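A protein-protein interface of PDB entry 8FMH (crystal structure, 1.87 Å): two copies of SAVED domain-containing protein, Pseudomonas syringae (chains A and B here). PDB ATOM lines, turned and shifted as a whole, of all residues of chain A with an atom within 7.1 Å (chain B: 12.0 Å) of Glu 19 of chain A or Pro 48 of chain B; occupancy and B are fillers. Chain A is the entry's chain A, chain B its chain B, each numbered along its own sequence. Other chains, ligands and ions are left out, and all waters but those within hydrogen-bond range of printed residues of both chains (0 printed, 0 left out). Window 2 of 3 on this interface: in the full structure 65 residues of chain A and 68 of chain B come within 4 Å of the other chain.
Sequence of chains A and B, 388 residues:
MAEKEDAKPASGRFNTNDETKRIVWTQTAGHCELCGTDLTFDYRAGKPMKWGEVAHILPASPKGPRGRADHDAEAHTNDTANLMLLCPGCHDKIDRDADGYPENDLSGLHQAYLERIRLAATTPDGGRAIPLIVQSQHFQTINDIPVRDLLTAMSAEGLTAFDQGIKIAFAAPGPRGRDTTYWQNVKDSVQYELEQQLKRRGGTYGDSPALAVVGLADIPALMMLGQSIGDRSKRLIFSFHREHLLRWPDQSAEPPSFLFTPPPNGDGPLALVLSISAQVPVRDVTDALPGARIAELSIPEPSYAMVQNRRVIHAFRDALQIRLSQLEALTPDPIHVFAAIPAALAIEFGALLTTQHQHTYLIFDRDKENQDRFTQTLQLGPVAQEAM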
ATOM      1  N   THR A  16      10.837   1.581   3.185  1.00  0.00           N
ATOM      2  CA  THR A  16      11.937   1.770   2.247  1.00  0.00           C
ATOM      3  C   THR A  16      11.540   2.739   1.142  1.00  0.00           C
ATOM      4  O   THR A  16      10.410   2.713   0.648  1.00  0.00           O
ATOM      5  CB  THR A  16      12.348   0.432   1.629  1.00  0.00           C
ATOM      6  OG1 THR A  16      12.379  -0.582   2.643  1.00  0.00           O
ATOM      7  CG2 THR A  16      13.725   0.548   0.983  1.00  0.00           C
ATOM      8  N   ASN A  17      12.480   3.588   0.745  1.00  0.00           N
ATOM      9  CA  ASN A  17      12.210   4.591  -0.271  1.00  0.00           C
ATOM     10  C   ASN A  17      12.568   4.064  -1.657  1.00  0.00           C
ATOM     11  O   ASN A  17      13.264   3.057  -1.810  1.00  0.00           O
ATOM     12  CB  ASN A  17      12.979   5.878   0.027  1.00  0.00           C
ATOM     13  CG  ASN A  17      14.422   5.816  -0.415  1.00  0.00           C
ATOM     14  OD1 ASN A  17      15.123   4.836  -0.173  1.00  0.00           O
ATOM     15  ND2 ASN A  17      14.874   6.875  -1.070  1.00  0.00           N
ATOM     16  N   ASP A  18      12.073   4.767  -2.679  1.00  0.00           N
ATOM     17  CA  ASP A  18      12.225   4.290  -4.051  1.00  0.00           C
ATOM     18  C   ASP A  18      13.689   4.213  -4.459  1.00  0.00           C
ATOM     19  O   ASP A  18      14.096   3.270  -5.148  1.00  0.00           O
ATOM     20  CB  ASP A  18      11.453   5.193  -5.011  1.00  0.00           C
ATOM     21  CG  ASP A  18       9.953   5.030  -4.884  1.00  0.00           C
ATOM     22  OD1 ASP A  18       9.508   3.944  -4.452  1.00  0.00           O
ATOM     23  OD2 ASP A  18       9.219   5.984  -5.225  1.00  0.00           O
ATOM     24  N   GLU A  19      14.498   5.200  -4.065  1.00  0.00           N
ATOM     25  CA  GLU A  19      15.913   5.155  -4.417  1.00  0.00           C
ATOM     26  C   GLU A  19      16.543   3.849  -3.956  1.00  0.00           C
ATOM     27  O   GLU A  19      17.306   3.222  -4.699  1.00  0.00           O
ATOM     28  CB  GLU A  19      16.654   6.342  -3.803  1.00  0.00           C
ATOM     29  CG  GLU A  19      18.130   6.418  -4.165  1.00  0.00           C
ATOM     30  CD  GLU A  19      18.821   7.611  -3.533  1.00  0.00           C
ATOM     31  OE1 GLU A  19      18.152   8.364  -2.793  1.00  0.00           O
ATOM     32  OE2 GLU A  19      20.033   7.795  -3.775  1.00  0.00           O
ATOM     33  N   THR A  20      16.220   3.417  -2.736  1.00  0.00           N
ATOM     34  CA  THR A  20      16.809   2.194  -2.205  1.00  0.00           C
ATOM     35  C   THR A  20      16.225   0.962  -2.883  1.00  0.00           C
ATOM     36  O   THR A  20      16.933  -0.029  -3.095  1.00  0.00           O
ATOM     37  CB  THR A  20      16.597   2.129  -0.696  1.00  0.00           C
ATOM     38  OG1 THR A  20      17.216   3.268  -0.084  1.00  0.00           O
ATOM     39  CG2 THR A  20      17.199   0.857  -0.120  1.00  0.00           C
ATOM     40  N   LYS A  21      14.936   1.001  -3.225  1.00  0.00           N
ATOM     41  CA  LYS A  21      14.345  -0.114  -3.956  1.00  0.00           C
ATOM     42  C   LYS A  21      14.984  -0.260  -5.332  1.00  0.00           C
ATOM     43  O   LYS A  21      15.239  -1.379  -5.790  1.00  0.00           O
ATOM     44  CB  LYS A  21      12.832   0.076  -4.062  1.00  0.00           C
ATOM     45  CG  LYS A  21      12.136  -0.055  -2.717  1.00  0.00           C
ATOM     46  CD  LYS A  21      10.619  -0.083  -2.822  1.00  0.00           C
ATOM     47  CE  LYS A  21       9.997  -0.357  -1.450  1.00  0.00           C
ATOM     48  NZ  LYS A  21       8.568  -0.790  -1.503  1.00  0.00           N
ATOM     49  N   ARG A  22      15.272   0.858  -5.998  1.00  0.00           N
ATOM     50  CA  ARG A  22      15.971   0.779  -7.276  1.00  0.00           C
ATOM     51  C   ARG A  22      17.378   0.221  -7.103  1.00  0.00           C
ATOM     52  O   ARG A  22      17.902  -0.435  -8.010  1.00  0.00           O
ATOM     53  CB  ARG A  22      16.015   2.157  -7.937  1.00  0.00           C
ATOM     54  CG  ARG A  22      16.454   2.130  -9.394  1.00  0.00           C
ATOM     55  CD  ARG A  22      16.141   3.440 -10.105  1.00  0.00           C
ATOM     56  NE  ARG A  22      16.711   3.479 -11.448  1.00  0.00           N
ATOM     57  CZ  ARG A  22      16.511   4.455 -12.324  1.00  0.00           C
ATOM     58  NH1 ARG A  22      15.745   5.497 -12.038  1.00  0.00           N
ATOM     59  NH2 ARG A  22      17.089   4.382 -13.519  1.00  0.00           N
ATOM     60  N   ILE A  23      17.999   0.459  -5.944  1.00  0.00           N
ATOM     61  CA  ILE A  23      19.336  -0.071  -5.685  1.00  0.00           C
ATOM     62  C   ILE A  23      19.279  -1.582  -5.505  1.00  0.00           C
ATOM     63  O   ILE A  23      20.106  -2.324  -6.052  1.00  0.00           O
ATOM     64  CB  ILE A  23      19.954   0.620  -4.456  1.00  0.00           C
ATOM     65  CG1 ILE A  23      20.382   2.050  -4.809  1.00  0.00           C
ATOM     66  CG2 ILE A  23      21.127  -0.188  -3.897  1.00  0.00           C
ATOM     67  CD1 ILE A  23      21.581   2.154  -5.757  1.00  0.00           C
ATOM     68  N   VAL A  24      18.313  -2.059  -4.718  1.00  0.00           N
ATOM     69  CA  VAL A  24      18.145  -3.498  -4.533  1.00  0.00           C
ATOM     70  C   VAL A  24      17.994  -4.184  -5.884  1.00  0.00           C
ATOM     71  O   VAL A  24      18.685  -5.162  -6.187  1.00  0.00           O
ATOM     72  CB  VAL A  24      16.939  -3.775  -3.616  1.00  0.00           C
ATOM     73  CG1 VAL A  24      16.564  -5.245  -3.634  1.00  0.00           C
ATOM     74  CG2 VAL A  24      17.243  -3.310  -2.194  1.00  0.00           C
ATOM     75  N   ASN A  78      16.263   1.275   5.089  1.00  0.00           N
ATOM     76  CA  ASN A  78      16.937   1.518   3.821  1.00  0.00           C
ATOM     77  C   ASN A  78      18.359   0.956   3.814  1.00  0.00           C
ATOM     78  O   ASN A  78      19.205   1.419   3.044  1.00  0.00           O
ATOM     79  CB  ASN A  78      16.947   3.017   3.515  1.00  0.00           C
ATOM     80  CG  ASN A  78      15.550   3.575   3.280  1.00  0.00           C
ATOM     81  OD1 ASN A  78      14.988   3.436   2.194  1.00  0.00           O
ATOM     82  ND2 ASN A  78      14.989   4.217   4.296  1.00  0.00           N
ATOM     83  N   ASP B  18      14.001   7.039 -19.738  1.00  0.00           N
ATOM     84  CA  ASP B  18      14.204   6.541 -18.381  1.00  0.00           C
ATOM     85  C   ASP B  18      13.971   5.037 -18.292  1.00  0.00           C
ATOM     86  O   ASP B  18      14.669   4.335 -17.551  1.00  0.00           O
ATOM     87  CB  ASP B  18      13.283   7.277 -17.409  1.00  0.00           C
ATOM     88  CG  ASP B  18      13.422   6.776 -15.988  1.00  0.00           C
ATOM     89  OD1 ASP B  18      14.541   6.860 -15.433  1.00  0.00           O
ATOM     90  OD2 ASP B  18      12.415   6.296 -15.424  1.00  0.00           O
ATOM     91  N   ARG B  22      16.830   2.225 -16.954  1.00  0.00           N
ATOM     92  CA  ARG B  22      16.557   1.313 -15.849  1.00  0.00           C
ATOM     93  C   ARG B  22      16.819  -0.133 -16.253  1.00  0.00           C
ATOM     94  O   ARG B  22      17.416  -0.903 -15.489  1.00  0.00           O
ATOM     95  CB  ARG B  22      15.114   1.496 -15.380  1.00  0.00           C
ATOM     96  CG  ARG B  22      14.840   1.013 -13.965  1.00  0.00           C
ATOM     97  CD  ARG B  22      13.429   1.380 -13.525  1.00  0.00           C
ATOM     98  NE  ARG B  22      12.494   1.348 -14.645  1.00  0.00           N
ATOM     99  CZ  ARG B  22      11.931   0.248 -15.130  1.00  0.00           C
ATOM    100  NH1 ARG B  22      12.159  -0.942 -14.597  1.00  0.00           N
ATOM    101  NH2 ARG B  22      11.122   0.344 -16.182  1.00  0.00           N
ATOM    102  N   TRP B  25      20.567  -0.613 -16.545  1.00  0.00           N
ATOM    103  CA  TRP B  25      21.196  -0.601 -15.228  1.00  0.00           C
ATOM    104  C   TRP B  25      20.958  -1.913 -14.493  1.00  0.00           C
ATOM    105  O   TRP B  25      21.877  -2.460 -13.871  1.00  0.00           O
ATOM    106  CB  TRP B  25      20.673   0.581 -14.408  1.00  0.00           C
ATOM    107  CG  TRP B  25      21.509   1.831 -14.534  1.00  0.00           C
ATOM    108  CD1 TRP B  25      21.471   2.752 -15.543  1.00  0.00           C
ATOM    109  CD2 TRP B  25      22.501   2.294 -13.608  1.00  0.00           C
ATOM    110  NE1 TRP B  25      22.378   3.757 -15.305  1.00  0.00           N
ATOM    111  CE2 TRP B  25      23.024   3.500 -14.124  1.00  0.00           C
ATOM    112  CE3 TRP B  25      22.999   1.807 -12.395  1.00  0.00           C
ATOM    113  CZ2 TRP B  25      24.020   4.224 -13.469  1.00  0.00           C
ATOM    114  CZ3 TRP B  25      23.989   2.528 -11.746  1.00  0.00           C
ATOM    115  CH2 TRP B  25      24.489   3.723 -12.284  1.00  0.00           C
ATOM    116  N   THR B  26      19.735  -2.444 -14.560  1.00  0.00           N
ATOM    117  CA  THR B  26      19.438  -3.687 -13.855  1.00  0.00           C
ATOM    118  C   THR B  26      20.133  -4.874 -14.516  1.00  0.00           C
ATOM    119  O   THR B  26      20.743  -5.705 -13.833  1.00  0.00           O
ATOM    120  CB  THR B  26      17.924  -3.911 -13.793  1.00  0.00           C
ATOM    121  OG1 THR B  26      17.316  -2.858 -13.034  1.00  0.00           O
ATOM    122  CG2 THR B  26      17.594  -5.249 -13.133  1.00  0.00           C
ATOM    123  N   GLY B  30      24.598  -2.475 -12.517  1.00  0.00           N
ATOM    124  CA  GLY B  30      25.127  -1.168 -12.183  1.00  0.00           C
ATOM    125  C   GLY B  30      26.623  -1.018 -12.308  1.00  0.00           C
ATOM    126  O   GLY B  30      27.181  -0.066 -11.759  1.00  0.00           O
ATOM    127  N   ASP B  38      31.873  -0.144  -9.919  1.00  0.00           N
ATOM    128  CA  ASP B  38      30.503  -0.009  -9.448  1.00  0.00           C
ATOM    129  C   ASP B  38      30.032   1.426  -9.639  1.00  0.00           C
ATOM    130  O   ASP B  38      30.711   2.374  -9.231  1.00  0.00           O
ATOM    131  CB  ASP B  38      30.408  -0.408  -7.978  1.00  0.00           C
ATOM    132  CG  ASP B  38      28.980  -0.630  -7.526  1.00  0.00           C
ATOM    133  OD1 ASP B  38      28.059  -0.074  -8.156  1.00  0.00           O
ATOM    134  OD2 ASP B  38      28.778  -1.361  -6.537  1.00  0.00           O
ATOM    135  N   LEU B  39      28.866   1.586 -10.261  1.00  0.00           N
ATOM    136  CA  LEU B  39      28.315   2.900 -10.562  1.00  0.00           C
ATOM    137  C   LEU B  39      27.178   3.291  -9.627  1.00  0.00           C
ATOM    138  O   LEU B  39      26.598   4.367  -9.795  1.00  0.00           O
ATOM    139  CB  LEU B  39      27.846   2.941 -12.019  1.00  0.00           C
ATOM    140  CG  LEU B  39      28.901   2.418 -13.004  1.00  0.00           C
ATOM    141  CD1 LEU B  39      28.432   2.518 -14.446  1.00  0.00           C
ATOM    142  CD2 LEU B  39      30.222   3.157 -12.835  1.00  0.00           C
ATOM    143  N   THR B  40      26.851   2.449  -8.648  1.00  0.00           N
ATOM    144  CA  THR B  40      25.915   2.789  -7.586  1.00  0.00           C
ATOM    145  C   THR B  40      26.612   3.407  -6.379  1.00  0.00           C
ATOM    146  O   THR B  40      26.014   3.483  -5.300  1.00  0.00           O
ATOM    147  CB  THR B  40      25.142   1.541  -7.144  1.00  0.00           C
ATOM    148  OG1 THR B  40      26.008   0.680  -6.393  1.00  0.00           O
ATOM    149  CG2 THR B  40      24.606   0.783  -8.353  1.00  0.00           C
ATOM    150  N   PHE B  41      27.863   3.843  -6.542  1.00  0.00           N
ATOM    151  CA  PHE B  41      28.651   4.341  -5.417  1.00  0.00           C
ATOM    152  C   PHE B  41      27.944   5.468  -4.675  1.00  0.00           C
ATOM    153  O   PHE B  41      28.068   5.586  -3.450  1.00  0.00           O
ATOM    154  CB  PHE B  41      30.010   4.821  -5.924  1.00  0.00           C
ATOM    155  CG  PHE B  41      29.924   5.893  -6.982  1.00  0.00           C
ATOM    156  CD1 PHE B  41      29.951   7.236  -6.631  1.00  0.00           C
ATOM    157  CD2 PHE B  41      29.815   5.560  -8.325  1.00  0.00           C
ATOM    158  CE1 PHE B  41      29.876   8.223  -7.598  1.00  0.00           C
ATOM    159  CE2 PHE B  41      29.740   6.547  -9.297  1.00  0.00           C
ATOM    160  CZ  PHE B  41      29.769   7.877  -8.930  1.00  0.00           C
ATOM    161  N   ASP B  42      27.215   6.319  -5.400  1.00  0.00           N
ATOM    162  CA  ASP B  42      26.568   7.463  -4.763  1.00  0.00           C
ATOM    163  C   ASP B  42      25.672   7.018  -3.614  1.00  0.00           C
ATOM    164  O   ASP B  42      25.740   7.568  -2.508  1.00  0.00           O
ATOM    165  CB  ASP B  42      25.767   8.254  -5.798  1.00  0.00           C
ATOM    166  CG  ASP B  42      26.638   9.168  -6.636  1.00  0.00           C
ATOM    167  OD1 ASP B  42      27.769   9.476  -6.202  1.00  0.00           O
ATOM    168  OD2 ASP B  42      26.185   9.589  -7.722  1.00  0.00           O
ATOM    169  N   TYR B  43      24.824   6.017  -3.855  1.00  0.00           N
ATOM    170  CA  TYR B  43      23.971   5.517  -2.784  1.00  0.00           C
ATOM    171  C   TYR B  43      24.799   4.899  -1.665  1.00  0.00           C
ATOM    172  O   TYR B  43      24.470   5.051  -0.483  1.00  0.00           O
ATOM    173  CB  TYR B  43      22.975   4.496  -3.332  1.00  0.00           C
ATOM    174  CG  TYR B  43      22.170   3.819  -2.249  1.00  0.00           C
ATOM    175  CD1 TYR B  43      20.991   4.384  -1.777  1.00  0.00           C
ATOM    176  CD2 TYR B  43      22.590   2.616  -1.693  1.00  0.00           C
ATOM    177  CE1 TYR B  43      20.253   3.770  -0.782  1.00  0.00           C
ATOM    178  CE2 TYR B  43      21.859   1.995  -0.696  1.00  0.00           C
ATOM    179  CZ  TYR B  43      20.691   2.577  -0.245  1.00  0.00           C
ATOM    180  OH  TYR B  43      19.956   1.966   0.744  1.00  0.00           O
ATOM    181  N   ARG B  44      25.879   4.195  -2.016  1.00  0.00           N
ATOM    182  CA  ARG B  44      26.674   3.503  -1.004  1.00  0.00           C
ATOM    183  C   ARG B  44      27.251   4.488   0.004  1.00  0.00           C
ATOM    184  O   ARG B  44      27.164   4.277   1.219  1.00  0.00           O
ATOM    185  CB  ARG B  44      27.797   2.703  -1.666  1.00  0.00           C
ATOM    186  CG  ARG B  44      27.352   1.766  -2.775  1.00  0.00           C
ATOM    187  CD  ARG B  44      26.248   0.831  -2.318  1.00  0.00           C
ATOM    188  NE  ARG B  44      25.962  -0.196  -3.312  1.00  0.00           N
ATOM    189  CZ  ARG B  44      24.978  -1.081  -3.216  1.00  0.00           C
ATOM    190  NH1 ARG B  44      24.152  -1.085  -2.182  1.00  0.00           N
ATOM    191  NH2 ARG B  44      24.819  -1.980  -4.181  1.00  0.00           N
ATOM    192  N   ALA B  45      27.853   5.573  -0.485  1.00  0.00           N
ATOM    193  CA  ALA B  45      28.460   6.549   0.414  1.00  0.00           C
ATOM    194  C   ALA B  45      27.407   7.238   1.275  1.00  0.00           C
ATOM    195  O   ALA B  45      27.650   7.525   2.453  1.00  0.00           O
ATOM    196  CB  ALA B  45      29.255   7.574  -0.393  1.00  0.00           C
ATOM    197  N   GLY B  46      26.232   7.506   0.706  1.00  0.00           N
ATOM    198  CA  GLY B  46      25.170   8.190   1.418  1.00  0.00           C
ATOM    199  C   GLY B  46      24.561   9.324   0.616  1.00  0.00           C
ATOM    200  O   GLY B  46      23.663  10.022   1.096  1.00  0.00           O
ATOM    201  N   LYS B  47      25.040   9.511  -0.613  1.00  0.00           N
ATOM    202  CA  LYS B  47      24.603  10.606  -1.462  1.00  0.00           C
ATOM    203  C   LYS B  47      23.414  10.185  -2.314  1.00  0.00           C
ATOM    204  O   LYS B  47      23.132   8.992  -2.465  1.00  0.00           O
ATOM    205  CB  LYS B  47      25.750  11.061  -2.360  1.00  0.00           C
ATOM    206  N   PRO B  48      22.693  11.145  -2.889  1.00  0.00           N
ATOM    207  CA  PRO B  48      21.538  10.795  -3.720  1.00  0.00           C
ATOM    208  C   PRO B  48      21.979  10.224  -5.056  1.00  0.00           C
ATOM    209  O   PRO B  48      22.990  10.637  -5.631  1.00  0.00           O
ATOM    210  CB  PRO B  48      20.811  12.131  -3.890  1.00  0.00           C
ATOM    211  CG  PRO B  48      21.907  13.139  -3.841  1.00  0.00           C
ATOM    212  CD  PRO B  48      22.931  12.599  -2.869  1.00  0.00           C
ATOM    213  N   MET B  49      21.204   9.268  -5.555  1.00  0.00           N
ATOM    214  CA  MET B  49      21.591   8.531  -6.750  1.00  0.00           C
ATOM    215  C   MET B  49      21.268   9.355  -7.991  1.00  0.00           C
ATOM    216  O   MET B  49      20.099   9.633  -8.275  1.00  0.00           O
ATOM    217  CB  MET B  49      20.887   7.178  -6.791  1.00  0.00           C
ATOM    218  CG  MET B  49      21.597   6.150  -7.645  1.00  0.00           C
ATOM    219  SD  MET B  49      23.299   5.877  -7.120  1.00  0.00           S
ATOM    220  CE  MET B  49      24.148   5.898  -8.697  1.00  0.00           C
ATOM    221  N   LYS B  50      22.308   9.743  -8.725  1.00  0.00           N
ATOM    222  CA  LYS B  50      22.189  10.462  -9.992  1.00  0.00           C
ATOM    223  C   LYS B  50      22.549   9.471 -11.098  1.00  0.00           C
ATOM    224  O   LYS B  50      23.694   9.409 -11.551  1.00  0.00           O
ATOM    225  CB  LYS B  50      23.094  11.691 -10.007  1.00  0.00           C
ATOM    226  CG  LYS B  50      22.803  12.682  -8.888  1.00  0.00           C
ATOM    227  CD  LYS B  50      21.550  13.500  -9.174  1.00  0.00           C
ATOM    228  CE  LYS B  50      20.807  13.856  -7.897  1.00  0.00           C
ATOM    229  NZ  LYS B  50      20.193  12.656  -7.268  1.00  0.00           N
ATOM    230  N   TRP B  51      21.551   8.699 -11.536  1.00  0.00           N
ATOM    231  CA  TRP B  51      21.804   7.596 -12.459  1.00  0.00           C
ATOM    232  C   TRP B  51      22.378   8.098 -13.780  1.00  0.00           C
ATOM    233  O   TRP B  51      23.344   7.532 -14.305  1.00  0.00           O
ATOM    234  CB  TRP B  51      20.510   6.813 -12.696  1.00  0.00           C
ATOM    235  CG  TRP B  51      19.835   6.353 -11.431  1.00  0.00           C
ATOM    236  CD1 TRP B  51      18.919   7.045 -10.690  1.00  0.00           C
ATOM    237  CD2 TRP B  51      20.021   5.098 -10.764  1.00  0.00           C
ATOM    238  NE1 TRP B  51      18.527   6.301  -9.603  1.00  0.00           N
ATOM    239  CE2 TRP B  51      19.188   5.100  -9.626  1.00  0.00           C
ATOM    240  CE3 TRP B  51      20.811   3.972 -11.019  1.00  0.00           C
ATOM    241  CZ2 TRP B  51      19.123   4.023  -8.745  1.00  0.00           C
ATOM    242  CZ3 TRP B  51      20.746   2.903 -10.142  1.00  0.00           C
ATOM    243  CH2 TRP B  51      19.909   2.938  -9.019  1.00  0.00           C
ATOM    244  N   GLY B  52      21.796   9.161 -14.334  1.00  0.00           N
ATOM    245  CA  GLY B  52      22.210   9.701 -15.616  1.00  0.00           C
ATOM    246  C   GLY B  52      23.433  10.593 -15.604  1.00  0.00           C
ATOM    247  O   GLY B  52      23.814  11.110 -16.657  1.00  0.00           O
ATOM    248  N   GLU B  53      24.061  10.797 -14.444  1.00  0.00           N
ATOM    249  CA  GLU B  53      25.313  11.536 -14.358  1.00  0.00           C
ATOM    250  C   GLU B  53      26.511  10.655 -14.040  1.00  0.00           C
ATOM    251  O   GLU B  53      27.638  11.025 -14.388  1.00  0.00           O
ATOM    252  CB  GLU B  53      25.209  12.633 -13.289  1.00  0.00           C
ATOM    253  N   VAL B  54      26.295   9.502 -13.397  1.00  0.00           N
ATOM    254  CA  VAL B  54      27.389   8.605 -13.029  1.00  0.00           C
ATOM    255  C   VAL B  54      27.743   7.614 -14.125  1.00  0.00           C
ATOM    256  O   VAL B  54      28.773   6.928 -14.016  1.00  0.00           O
ATOM    257  CB  VAL B  54      27.052   7.803 -11.754  1.00  0.00           C
ATOM    258  CG1 VAL B  54      26.799   8.737 -10.587  1.00  0.00           C
ATOM    259  CG2 VAL B  54      25.845   6.896 -11.984  1.00  0.00           C
ATOM    260  N   ALA B  55      26.930   7.504 -15.173  1.00  0.00           N
ATOM    261  CA  ALA B  55      27.133   6.472 -16.177  1.00  0.00           C
ATOM    262  C   ALA B  55      26.511   6.918 -17.490  1.00  0.00           C
ATOM    263  O   ALA B  55      25.605   7.757 -17.519  1.00  0.00           O
ATOM    264  CB  ALA B  55      26.532   5.136 -15.731  1.00  0.00           C
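Arg 22 of chain A touches Asp 18 of chain B, but with the chains exchanged Asp 18 of chain A does not touch Arg 22 of chain B (8.6 Å). Arg 22 of chain A touches its own counterpart, Arg 22 of chain B. 2 positions are printed for both chains. Of the 12 pairs that touch across the chains among the printed residues, 1 has its exchanged pair printed and touching as well.
ND2 of Asn 17 of chain A sits close to N of Glu 19 of chain A (3.5 Å). OD1 of Asn 17 of chain A sits at hydrogen-bond distance from OG1 of Thr 20 of chain A (2.6 Å). The side-chain amide oxygen of Asn 78 of chain A lies close to the side-chain amide oxygen of Asn 17 of chain A (2.8 Å). The backbone carbonyl oxygen (O) of Arg 22 of chain B is in hydrogen-bond range of the side-chain hydroxyl (OG1) of Thr 26 of chain B (3.1 Å). The side-chain carboxylate (OD1) of Asp 38 of chain B is in hydrogen-bond range of the side-chain hydroxyl (OG1) of Thr 40 of chain B (2.8 Å). N of Lys 47 of chain B sits at hydrogen-bond distance from O of Asp 42 of chain B, at 2.8 Å.
Of the 23 printed residues of chain B, 9 touch a printed residue of chain A. Hydrophobic or aromatic side chains of chain B that line the printed part of chain A: Tyr 43, Met 49 and Trp 51. Along chain B the printed residues that touch a printed residue of chain A span positions 18 to 51. Among the printed residues, 12 pairs touch across the chains.
No residue of chain B comes within 4 Å of Asp 18 of chain A. Printed residues of chain B within 4 Å of Glu 19 of chain A: Lys 47 (3.6 Å), Pro 48 (3.4 Å) and Met 49 (2.6 Å). Of chain B, only Thr 40 (3.9 Å), Tyr 43 (3.6 Å), Arg 44 (3.6 Å) and Trp 51 (3.7 Å) come within 4 Å of Ile 23 of chain A. Of the printed residues of chain A, Asp 18 of chain B touches Arg 22 (3.9 Å). Of the printed residues of chain A, Arg 22 of chain B touches Arg 22 (3.9 Å). Of the printed residues of chain A, Tyr 43 of chain B touches Thr 20 (3.1 Å), Ile 23 (3.6 Å) and Asn 78 (2.5 Å). Of chain A, only Glu 19 comes within 4 Å of Pro 48 of chain B. Of the printed residues of chain A, Met 49 of chain B touches Glu 19 (2.6 Å). The nearest printed residue of chain A that does not touch Tyr 43 of chain B is Glu 19 of chain A (4.1 Å).
The backbone NH (N) of Met 49 of chain B lies within hydrogen-bond range of the side-chain carboxylate (OE2) of Glu 19 of chain A (2.6 Å). OH of Tyr 43 of chain B sits close to OG1 of Thr 20 of chain A, at 3.1 Å. The side-chain carboxylate (OD1) of Asp 18 of chain B lies within salt-bridge range of the guanidinium group (NH1) of Arg 22 of chain A (3.9 Å). O of Asn 78 of chain A lies within hydrogen-bond range of OH of Tyr 43 of chain B, 2.5 Å away.
Glu 19 of chain A touches Lys 47 of chain B (OE2 to O, 3.6 Å). OE2 of Glu 19 of chain A touches CA of Pro 48 of chain B (3.4 Å). Arg 22 of chain A touches Arg 22 of chain B. Arg 22 of chain A touches Trp 51 of chain B (CD to CZ2, 3.3 Å). Ile 23 of chain A touches Thr 40 of chain B (CD1 to CB, 3.9 Å). Tyr 43 of chain B touches Ile 23 of chain A (CG to CG1, 3.6 Å). Ile 23 of chain A touches Arg 44 of chain B. Ile 23 of chain A touches Trp 51 of chain B (CD1 to CH2, 3.7 Å).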
